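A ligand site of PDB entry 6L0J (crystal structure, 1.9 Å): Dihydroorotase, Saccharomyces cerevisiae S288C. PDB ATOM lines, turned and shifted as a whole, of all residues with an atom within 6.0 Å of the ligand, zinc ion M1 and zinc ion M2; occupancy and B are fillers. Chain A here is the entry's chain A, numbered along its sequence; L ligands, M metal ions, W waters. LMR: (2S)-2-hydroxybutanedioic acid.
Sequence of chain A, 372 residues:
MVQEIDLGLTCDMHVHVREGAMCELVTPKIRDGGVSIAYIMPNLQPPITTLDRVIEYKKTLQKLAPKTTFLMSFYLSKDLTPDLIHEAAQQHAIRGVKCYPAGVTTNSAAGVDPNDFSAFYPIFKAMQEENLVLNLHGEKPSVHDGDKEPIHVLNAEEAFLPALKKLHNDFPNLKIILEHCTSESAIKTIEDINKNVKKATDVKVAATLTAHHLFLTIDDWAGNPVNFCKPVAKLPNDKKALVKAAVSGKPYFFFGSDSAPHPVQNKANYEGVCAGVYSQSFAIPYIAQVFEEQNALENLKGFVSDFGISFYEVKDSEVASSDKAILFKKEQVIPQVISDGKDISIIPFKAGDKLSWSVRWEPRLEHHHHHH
OG1 of Thr 105 is in hydrogen-bond range of O1B of the ligand. The guanidinium group of Arg 18 is in salt-bridge range of an oxygen (O4B) of the ligand (2.5 Å). O4B of the ligand lies within hydrogen-bond range of ND2 of Asn 43, at 2.5 Å. The side-chain hydroxyl (OG1) of Thr 106 sits at hydrogen-bond distance from an oxygen (O4A) of the ligand, 2.9 Å away. The backbone carbonyl oxygen (O) of Ala 275 is in hydrogen-bond range of an oxygen (O2) of the ligand. NE2 of His 262 is in hydrogen-bond range of O4A of the ligand, at 3.3 Å.
NZ of KCX 98 sits at hydrogen-bond distance from the side-chain hydroxyl (OH) of Tyr 100, at 3.0 Å. ND1 of His 14 sits at hydrogen-bond distance from OE1 of Glu 179, at 2.9 Å. OD1 of Asn 43 sits at hydrogen-bond distance from ND1 of His 16 (2.8 Å). The guanidinium group (NH2) of Arg 18 sits at hydrogen-bond distance from a ring nitrogen (NE2) of His 262 (3.2 Å). The guanidinium group of Arg 18 lies within hydrogen-bond range of the backbone carbonyl oxygen of Pro 261 (2.8 Å). The side-chain amide nitrogen (ND2) of Asn 43 is in hydrogen-bond range of the backbone carbonyl oxygen (O) of Thr 106 (3.2 Å). O of Asn 43 sits at hydrogen-bond distance from ND2 of Asn 107 (2.7 Å). NE2 of His 262 lies within hydrogen-bond range of O of Ala 275, at 2.7 Å.
Merely in contact with the ligand: Lys 230 and Ala 260. Within 4 Å of the ligand: His 14, His 16, Arg 18, Asn 43, KCX 98, Thr 105, Thr 106, His 137, His 180, Lys 230, Asp 258, Ala 260, His 262 and Ala 275.
Within 4 Å of zinc ion M1: His 14, His 16, KCX 98 and Asp 258.
Of the 24 residues printed, 3 come within 4 Å of zinc ion M2.
Zinc ion M1 is bound by NE2 of His 14, OD1 of Asp 258, OQ2 of KCX 98, O1A of the ligand and NE2 of His 16.
OQ1 of KCX 98 is bound to zinc ion M2 (2.0 Å). Zinc ion M2 is bound by a ring nitrogen (ND1) of His 137. A ring nitrogen (NE2) of His 180 is bound to zinc ion M2 (2.1 Å). O1A of the ligand binds zinc ion M2 (2.5 Å). Slightly farther from zinc ion M2 lies O1B of the ligand (2.8 Å).
Water W1 lies within hydrogen-bond range of the backbone carbonyl oxygen of Lys 230 (2.7 Å), an oxygen (O2) of the ligand (2.8 Å) and the side-chain carboxylate of Asp 258 (3.0 Å).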
ATOM      1  N   HIS A  14     -15.732  13.445 -20.588  1.00  0.00           N
ATOM      2  CA  HIS A  14     -15.144  14.130 -21.753  1.00  0.00           C
ATOM      3  C   HIS A  14     -14.156  13.175 -22.427  1.00  0.00           C
ATOM      4  O   HIS A  14     -12.967  13.175 -22.101  1.00  0.00           O
ATOM      5  CB  HIS A  14     -14.484  15.443 -21.348  1.00  0.00           C
ATOM      6  CG  HIS A  14     -14.101  16.324 -22.500  1.00  0.00           C
ATOM      7  ND1 HIS A  14     -14.279  17.693 -22.496  1.00  0.00           N
ATOM      8  CD2 HIS A  14     -13.562  16.022 -23.712  1.00  0.00           C
ATOM      9  CE1 HIS A  14     -13.855  18.196 -23.651  1.00  0.00           C
ATOM     10  NE2 HIS A  14     -13.414  17.199 -24.400  1.00  0.00           N
ATOM     11  N   HIS A  16     -12.723  11.351 -26.119  1.00  0.00           N
ATOM     12  CA  HIS A  16     -12.587  11.183 -27.565  1.00  0.00           C
ATOM     13  C   HIS A  16     -12.117   9.774 -27.879  1.00  0.00           C
ATOM     14  O   HIS A  16     -11.081   9.331 -27.360  1.00  0.00           O
ATOM     15  CB  HIS A  16     -11.602  12.199 -28.160  1.00  0.00           C
ATOM     16  CG  HIS A  16     -11.994  13.619 -27.932  1.00  0.00           C
ATOM     17  ND1 HIS A  16     -12.707  14.351 -28.848  1.00  0.00           N
ATOM     18  CD2 HIS A  16     -11.762  14.446 -26.879  1.00  0.00           C
ATOM     19  CE1 HIS A  16     -12.899  15.577 -28.378  1.00  0.00           C
ATOM     20  NE2 HIS A  16     -12.331  15.656 -27.191  1.00  0.00           N
ATOM     21  N   ARG A  18     -12.390   8.684 -31.405  1.00  0.00           N
ATOM     22  CA  ARG A  18     -12.086   8.731 -32.844  1.00  0.00           C
ATOM     23  C   ARG A  18     -12.928   7.660 -33.570  1.00  0.00           C
ATOM     24  O   ARG A  18     -14.045   7.341 -33.155  1.00  0.00           O
ATOM     25  CB  ARG A  18     -10.581   8.577 -33.080  1.00  0.00           C
ATOM     26  CG  ARG A  18      -9.676   9.424 -32.164  1.00  0.00           C
ATOM     27  CD  ARG A  18      -9.884  10.949 -32.370  1.00  0.00           C
ATOM     28  NE  ARG A  18      -8.832  11.683 -31.673  1.00  0.00           N
ATOM     29  CZ  ARG A  18      -8.947  12.924 -31.212  1.00  0.00           C
ATOM     30  NH1 ARG A  18     -10.083  13.609 -31.368  1.00  0.00           N
ATOM     31  NH2 ARG A  18      -7.902  13.483 -30.612  1.00  0.00           N
ATOM     32  N   MET A  41     -17.418  12.687 -27.171  1.00  0.00           N
ATOM     33  CA  MET A  41     -17.417  13.946 -27.904  1.00  0.00           C
ATOM     34  C   MET A  41     -17.595  13.710 -29.399  1.00  0.00           C
ATOM     35  O   MET A  41     -17.274  12.640 -29.917  1.00  0.00           O
ATOM     36  CB  MET A  41     -16.122  14.704 -27.637  1.00  0.00           C
ATOM     37  CG  MET A  41     -16.070  15.254 -26.206  1.00  0.00           C
ATOM     38  SD  MET A  41     -17.506  16.348 -25.894  1.00  0.00           S
ATOM     39  CE  MET A  41     -17.440  16.556 -24.101  1.00  0.00           C
ATOM     40  N   ASN A  43     -16.510  15.532 -32.317  1.00  0.00           N
ATOM     41  CA  ASN A  43     -15.646  16.185 -33.305  1.00  0.00           C
ATOM     42  C   ASN A  43     -14.920  15.175 -34.208  1.00  0.00           C
ATOM     43  O   ASN A  43     -13.684  15.169 -34.331  1.00  0.00           O
ATOM     44  CB  ASN A  43     -14.663  17.112 -32.604  1.00  0.00           C
ATOM     45  CG  ASN A  43     -13.685  16.364 -31.704  1.00  0.00           C
ATOM     46  OD1 ASN A  43     -14.023  15.304 -31.158  1.00  0.00           O
ATOM     47  ND2 ASN A  43     -12.464  16.880 -31.560  1.00  0.00           N
ATOM     48  N   KCX A  98     -22.150  19.575 -28.073  1.00  0.00           N
ATOM     49  CA  KCX A  98     -20.861  20.178 -27.746  1.00  0.00           C
ATOM     50  CB  KCX A  98     -19.760  19.102 -27.786  1.00  0.00           C
ATOM     51  CG  KCX A  98     -18.314  19.629 -27.719  1.00  0.00           C
ATOM     52  CD  KCX A  98     -18.006  20.147 -26.318  1.00  0.00           C
ATOM     53  CE  KCX A  98     -16.560  20.481 -26.231  1.00  0.00           C
ATOM     54  NZ  KCX A  98     -15.790  19.271 -26.619  1.00  0.00           N
ATOM     55  C   KCX A  98     -20.530  21.306 -28.711  1.00  0.00           C
ATOM     56  O   KCX A  98     -20.588  21.138 -29.935  1.00  0.00           O
ATOM     57  CX  KCX A  98     -14.460  19.273 -26.540  1.00  0.00           C
ATOM     58  OQ1 KCX A  98     -13.846  20.286 -26.103  1.00  0.00           O
ATOM     59  OQ2 KCX A  98     -13.844  18.248 -26.885  1.00  0.00           O
ATOM     60  N   TYR A 100     -17.751  23.778 -30.339  1.00  0.00           N
ATOM     61  CA  TYR A 100     -16.366  24.098 -30.667  1.00  0.00           C
ATOM     62  C   TYR A 100     -16.345  25.442 -31.364  1.00  0.00           C
ATOM     63  O   TYR A 100     -16.861  25.556 -32.492  1.00  0.00           O
ATOM     64  CB  TYR A 100     -15.756  23.037 -31.595  1.00  0.00           C
ATOM     65  CG  TYR A 100     -15.667  21.657 -30.967  1.00  0.00           C
ATOM     66  CD1 TYR A 100     -14.538  21.287 -30.241  1.00  0.00           C
ATOM     67  CD2 TYR A 100     -16.685  20.752 -31.105  1.00  0.00           C
ATOM     68  CE1 TYR A 100     -14.448  20.034 -29.660  1.00  0.00           C
ATOM     69  CE2 TYR A 100     -16.607  19.475 -30.533  1.00  0.00           C
ATOM     70  CZ  TYR A 100     -15.477  19.126 -29.816  1.00  0.00           C
ATOM     71  OH  TYR A 100     -15.389  17.893 -29.221  1.00  0.00           O
ATOM     72  N   VAL A 104     -10.317  26.693 -32.995  1.00  0.00           N
ATOM     73  CA  VAL A 104      -9.520  26.677 -31.772  1.00  0.00           C
ATOM     74  C   VAL A 104      -8.960  25.300 -31.427  1.00  0.00           C
ATOM     75  O   VAL A 104      -8.066  25.210 -30.565  1.00  0.00           O
ATOM     76  CB  VAL A 104     -10.274  27.217 -30.530  1.00  0.00           C
ATOM     77  CG1 VAL A 104     -10.819  28.630 -30.793  1.00  0.00           C
ATOM     78  CG2 VAL A 104     -11.405  26.290 -30.105  1.00  0.00           C
ATOM     79  N   THR A 105      -9.450  24.225 -32.035  1.00  0.00           N
ATOM     80  CA  THR A 105      -8.918  22.907 -31.657  1.00  0.00           C
ATOM     81  C   THR A 105      -9.190  21.870 -32.741  1.00  0.00           C
ATOM     82  O   THR A 105      -9.652  22.197 -33.841  1.00  0.00           O
ATOM     83  CB  THR A 105      -9.503  22.464 -30.301  1.00  0.00           C
ATOM     84  OG1 THR A 105      -8.784  21.299 -29.846  1.00  0.00           O
ATOM     85  CG2 THR A 105     -11.001  22.157 -30.414  1.00  0.00           C
ATOM     86  N   THR A 106      -8.881  20.614 -32.430  1.00  0.00           N
ATOM     87  CA  THR A 106      -8.992  19.510 -33.379  1.00  0.00           C
ATOM     88  C   THR A 106     -10.387  19.427 -33.999  1.00  0.00           C
ATOM     89  O   THR A 106     -11.383  19.356 -33.284  1.00  0.00           O
ATOM     90  CB  THR A 106      -8.686  18.187 -32.682  1.00  0.00           C
ATOM     91  OG1 THR A 106      -7.369  18.247 -32.093  1.00  0.00           O
ATOM     92  CG2 THR A 106      -8.812  17.007 -33.672  1.00  0.00           C
ATOM     93  N   ASN A 107     -10.446  19.418 -35.328  1.00  0.00           N
ATOM     94  CA  ASN A 107     -11.705  19.215 -36.051  1.00  0.00           C
ATOM     95  C   ASN A 107     -12.737  20.269 -35.680  1.00  0.00           C
ATOM     96  O   ASN A 107     -13.922  19.965 -35.515  1.00  0.00           O
ATOM     97  CB  ASN A 107     -12.263  17.806 -35.809  1.00  0.00           C
ATOM     98  CG  ASN A 107     -11.409  16.708 -36.418  1.00  0.00           C
ATOM     99  OD1 ASN A 107     -10.598  16.969 -37.297  1.00  0.00           O
ATOM    100  ND2 ASN A 107     -11.576  15.469 -35.953  1.00  0.00           N
ATOM    101  N   HIS A 137     -16.414  24.049 -25.330  1.00  0.00           N
ATOM    102  CA  HIS A 137     -14.961  24.292 -25.403  1.00  0.00           C
ATOM    103  C   HIS A 137     -14.816  25.809 -25.356  1.00  0.00           C
ATOM    104  O   HIS A 137     -14.898  26.507 -26.366  1.00  0.00           O
ATOM    105  CB  HIS A 137     -14.326  23.694 -26.665  1.00  0.00           C
ATOM    106  CG  HIS A 137     -12.832  23.906 -26.753  1.00  0.00           C
ATOM    107  ND1 HIS A 137     -11.919  22.865 -26.732  1.00  0.00           N
ATOM    108  CD2 HIS A 137     -12.097  25.047 -26.817  1.00  0.00           C
ATOM    109  CE1 HIS A 137     -10.687  23.359 -26.779  1.00  0.00           C
ATOM    110  NE2 HIS A 137     -10.773  24.681 -26.837  1.00  0.00           N
ATOM    111  N   GLU A 179     -16.077  22.903 -20.310  1.00  0.00           N
ATOM    112  CA  GLU A 179     -15.228  21.731 -20.363  1.00  0.00           C
ATOM    113  C   GLU A 179     -13.793  22.117 -20.030  1.00  0.00           C
ATOM    114  O   GLU A 179     -13.374  23.244 -20.233  1.00  0.00           O
ATOM    115  CB  GLU A 179     -15.256  21.102 -21.773  1.00  0.00           C
ATOM    116  CG  GLU A 179     -16.592  20.484 -22.174  1.00  0.00           C
ATOM    117  CD  GLU A 179     -17.042  19.344 -21.239  1.00  0.00           C
ATOM    118  OE1 GLU A 179     -16.180  18.711 -20.593  1.00  0.00           O
ATOM    119  OE2 GLU A 179     -18.251  19.094 -21.138  1.00  0.00           O
ATOM    120  N   HIS A 180     -13.029  21.125 -19.561  1.00  0.00           N
ATOM    121  CA  HIS A 180     -11.595  21.220 -19.298  1.00  0.00           C
ATOM    122  C   HIS A 180     -11.099  22.624 -18.939  1.00  0.00           C
ATOM    123  O   HIS A 180     -10.405  23.277 -19.730  1.00  0.00           O
ATOM    124  CB  HIS A 180     -10.785  20.640 -20.487  1.00  0.00           C
ATOM    125  CG  HIS A 180     -11.221  21.096 -21.860  1.00  0.00           C
ATOM    126  ND1 HIS A 180     -11.578  22.387 -22.179  1.00  0.00           N
ATOM    127  CD2 HIS A 180     -11.285  20.401 -23.035  1.00  0.00           C
ATOM    128  CE1 HIS A 180     -11.860  22.474 -23.468  1.00  0.00           C
ATOM    129  NE2 HIS A 180     -11.696  21.274 -24.012  1.00  0.00           N
ATOM    130  N   CYS A 229      -1.938  20.410 -25.815  1.00  0.00           N
ATOM    131  CA  CYS A 229      -3.371  20.205 -25.930  1.00  0.00           C
ATOM    132  C   CYS A 229      -4.016  21.581 -25.993  1.00  0.00           C
ATOM    133  O   CYS A 229      -3.349  22.617 -25.831  1.00  0.00           O
ATOM    134  CB  CYS A 229      -3.918  19.357 -24.765  1.00  0.00           C
ATOM    135  SG  CYS A 229      -3.753  20.131 -23.088  1.00  0.00           S
ATOM    136  N   LYS A 230      -5.318  21.604 -26.299  1.00  0.00           N
ATOM    137  CA  LYS A 230      -6.157  22.784 -26.152  1.00  0.00           C
ATOM    138  C   LYS A 230      -7.236  22.504 -25.117  1.00  0.00           C
ATOM    139  O   LYS A 230      -7.793  21.396 -25.088  1.00  0.00           O
ATOM    140  CB  LYS A 230      -6.820  23.196 -27.488  1.00  0.00           C
ATOM    141  CG  LYS A 230      -5.843  23.617 -28.602  1.00  0.00           C
ATOM    142  CD  LYS A 230      -4.828  24.703 -28.179  1.00  0.00           C
ATOM    143  CE  LYS A 230      -5.478  26.041 -27.924  1.00  0.00           C
ATOM    144  NZ  LYS A 230      -6.003  26.641 -29.191  1.00  0.00           N
ATOM    145  N   PRO A 231      -7.543  23.473 -24.212  1.00  0.00           N
ATOM    146  CA  PRO A 231      -6.822  24.723 -24.045  1.00  0.00           C
ATOM    147  C   PRO A 231      -5.433  24.373 -23.506  1.00  0.00           C
ATOM    148  O   PRO A 231      -5.328  23.328 -22.876  1.00  0.00           O
ATOM    149  CB  PRO A 231      -7.656  25.520 -22.993  1.00  0.00           C
ATOM    150  CG  PRO A 231      -8.939  24.707 -22.815  1.00  0.00           C
ATOM    151  CD  PRO A 231      -8.566  23.279 -23.170  1.00  0.00           C
ATOM    152  N   ASP A 258     -10.770  14.606 -21.239  1.00  0.00           N
ATOM    153  CA  ASP A 258     -10.350  15.039 -22.572  1.00  0.00           C
ATOM    154  C   ASP A 258      -9.209  14.157 -23.073  1.00  0.00           C
ATOM    155  O   ASP A 258      -8.276  14.657 -23.715  1.00  0.00           O
ATOM    156  CB  ASP A 258      -9.919  16.509 -22.620  1.00  0.00           C
ATOM    157  CG  ASP A 258      -9.886  17.075 -24.057  1.00  0.00           C
ATOM    158  OD1 ASP A 258     -10.624  16.533 -24.918  1.00  0.00           O
ATOM    159  OD2 ASP A 258      -9.123  18.025 -24.351  1.00  0.00           O
ATOM    160  N   SER A 259      -9.286  12.846 -22.836  1.00  0.00           N
ATOM    161  CA  SER A 259      -8.326  11.970 -23.486  1.00  0.00           C
ATOM    162  C   SER A 259      -8.525  12.083 -24.989  1.00  0.00           C
ATOM    163  O   SER A 259      -9.621  11.872 -25.492  1.00  0.00           O
ATOM    164  CB  SER A 259      -8.486  10.527 -23.019  1.00  0.00           C
ATOM    165  OG  SER A 259      -7.555   9.698 -23.707  1.00  0.00           O
ATOM    166  N   ALA A 260      -7.470  12.486 -25.687  1.00  0.00           N
ATOM    167  CA  ALA A 260      -7.556  12.936 -27.084  1.00  0.00           C
ATOM    168  C   ALA A 260      -6.461  12.235 -27.881  1.00  0.00           C
ATOM    169  O   ALA A 260      -5.387  12.795 -28.108  1.00  0.00           O
ATOM    170  CB  ALA A 260      -7.407  14.444 -27.189  1.00  0.00           C
ATOM    171  N   PRO A 261      -6.713  11.008 -28.317  1.00  0.00           N
ATOM    172  CA  PRO A 261      -5.626  10.227 -28.921  1.00  0.00           C
ATOM    173  C   PRO A 261      -5.282  10.656 -30.339  1.00  0.00           C
ATOM    174  O   PRO A 261      -6.146  10.936 -31.170  1.00  0.00           O
ATOM    175  CB  PRO A 261      -6.167   8.784 -28.888  1.00  0.00           C
ATOM    176  CG  PRO A 261      -7.616   8.900 -28.755  1.00  0.00           C
ATOM    177  CD  PRO A 261      -7.892  10.190 -28.022  1.00  0.00           C
ATOM    178  N   HIS A 262      -3.975  10.727 -30.597  1.00  0.00           N
ATOM    179  CA  HIS A 262      -3.417  10.971 -31.903  1.00  0.00           C
ATOM    180  C   HIS A 262      -2.278   9.989 -32.125  1.00  0.00           C
ATOM    181  O   HIS A 262      -1.548   9.681 -31.181  1.00  0.00           O
ATOM    182  CB  HIS A 262      -2.855  12.401 -32.033  1.00  0.00           C
ATOM    183  CG  HIS A 262      -3.886  13.470 -31.914  1.00  0.00           C
ATOM    184  ND1 HIS A 262      -4.754  13.786 -32.938  1.00  0.00           N
ATOM    185  CD2 HIS A 262      -4.189  14.308 -30.895  1.00  0.00           C
ATOM    186  CE1 HIS A 262      -5.553  14.769 -32.553  1.00  0.00           C
ATOM    187  NE2 HIS A 262      -5.234  15.093 -31.311  1.00  0.00           N
ATOM    188  N   ALA A 275      -3.283  18.885 -31.413  1.00  0.00           N
ATOM    189  CA  ALA A 275      -3.518  19.161 -30.009  1.00  0.00           C
ATOM    190  C   ALA A 275      -4.203  17.967 -29.364  1.00  0.00           C
ATOM    191  O   ALA A 275      -5.183  17.454 -29.907  1.00  0.00           O
ATOM    192  CB  ALA A 275      -4.384  20.400 -29.850  1.00  0.00           C
ATOM    193  N   GLY A 276      -3.729  17.541 -28.200  1.00  0.00           N
ATOM    194  CA  GLY A 276      -4.384  16.432 -27.509  1.00  0.00           C
ATOM    195  C   GLY A 276      -3.444  15.533 -26.713  1.00  0.00           C
ATOM    196  O   GLY A 276      -2.368  15.159 -27.186  1.00  0.00           O
HETATM  197  C1  LMR L   1     -10.096  19.216 -27.638  1.00  0.00           C
HETATM  198  O1A LMR L   1     -10.885  18.852 -26.715  1.00  0.00           O
HETATM  199  O1B LMR L   1      -9.888  20.446 -27.750  1.00  0.00           O
HETATM  200  C2  LMR L   1      -9.408  18.293 -28.674  1.00  0.00           C
HETATM  201  O2  LMR L   1      -7.970  18.272 -28.714  1.00  0.00           O
HETATM  202  C3  LMR L   1      -9.758  16.868 -28.460  1.00  0.00           C
HETATM  203  C4  LMR L   1      -9.380  16.305 -29.827  1.00  0.00           C
HETATM  204  O4A LMR L   1      -8.168  16.221 -30.233  1.00  0.00           O
HETATM  205  O4B LMR L   1     -10.347  15.974 -30.510  1.00  0.00           O
HETATM  206 ZN    ZN M   1     -12.177  17.372 -25.981  1.00  0.00          ZN
HETATM  207 ZN    ZN M   2     -11.996  20.936 -26.050  1.00  0.00          ZN
HETATM  208  O   HOH W   1      -6.999  19.027 -26.158  1.00  0.00           O
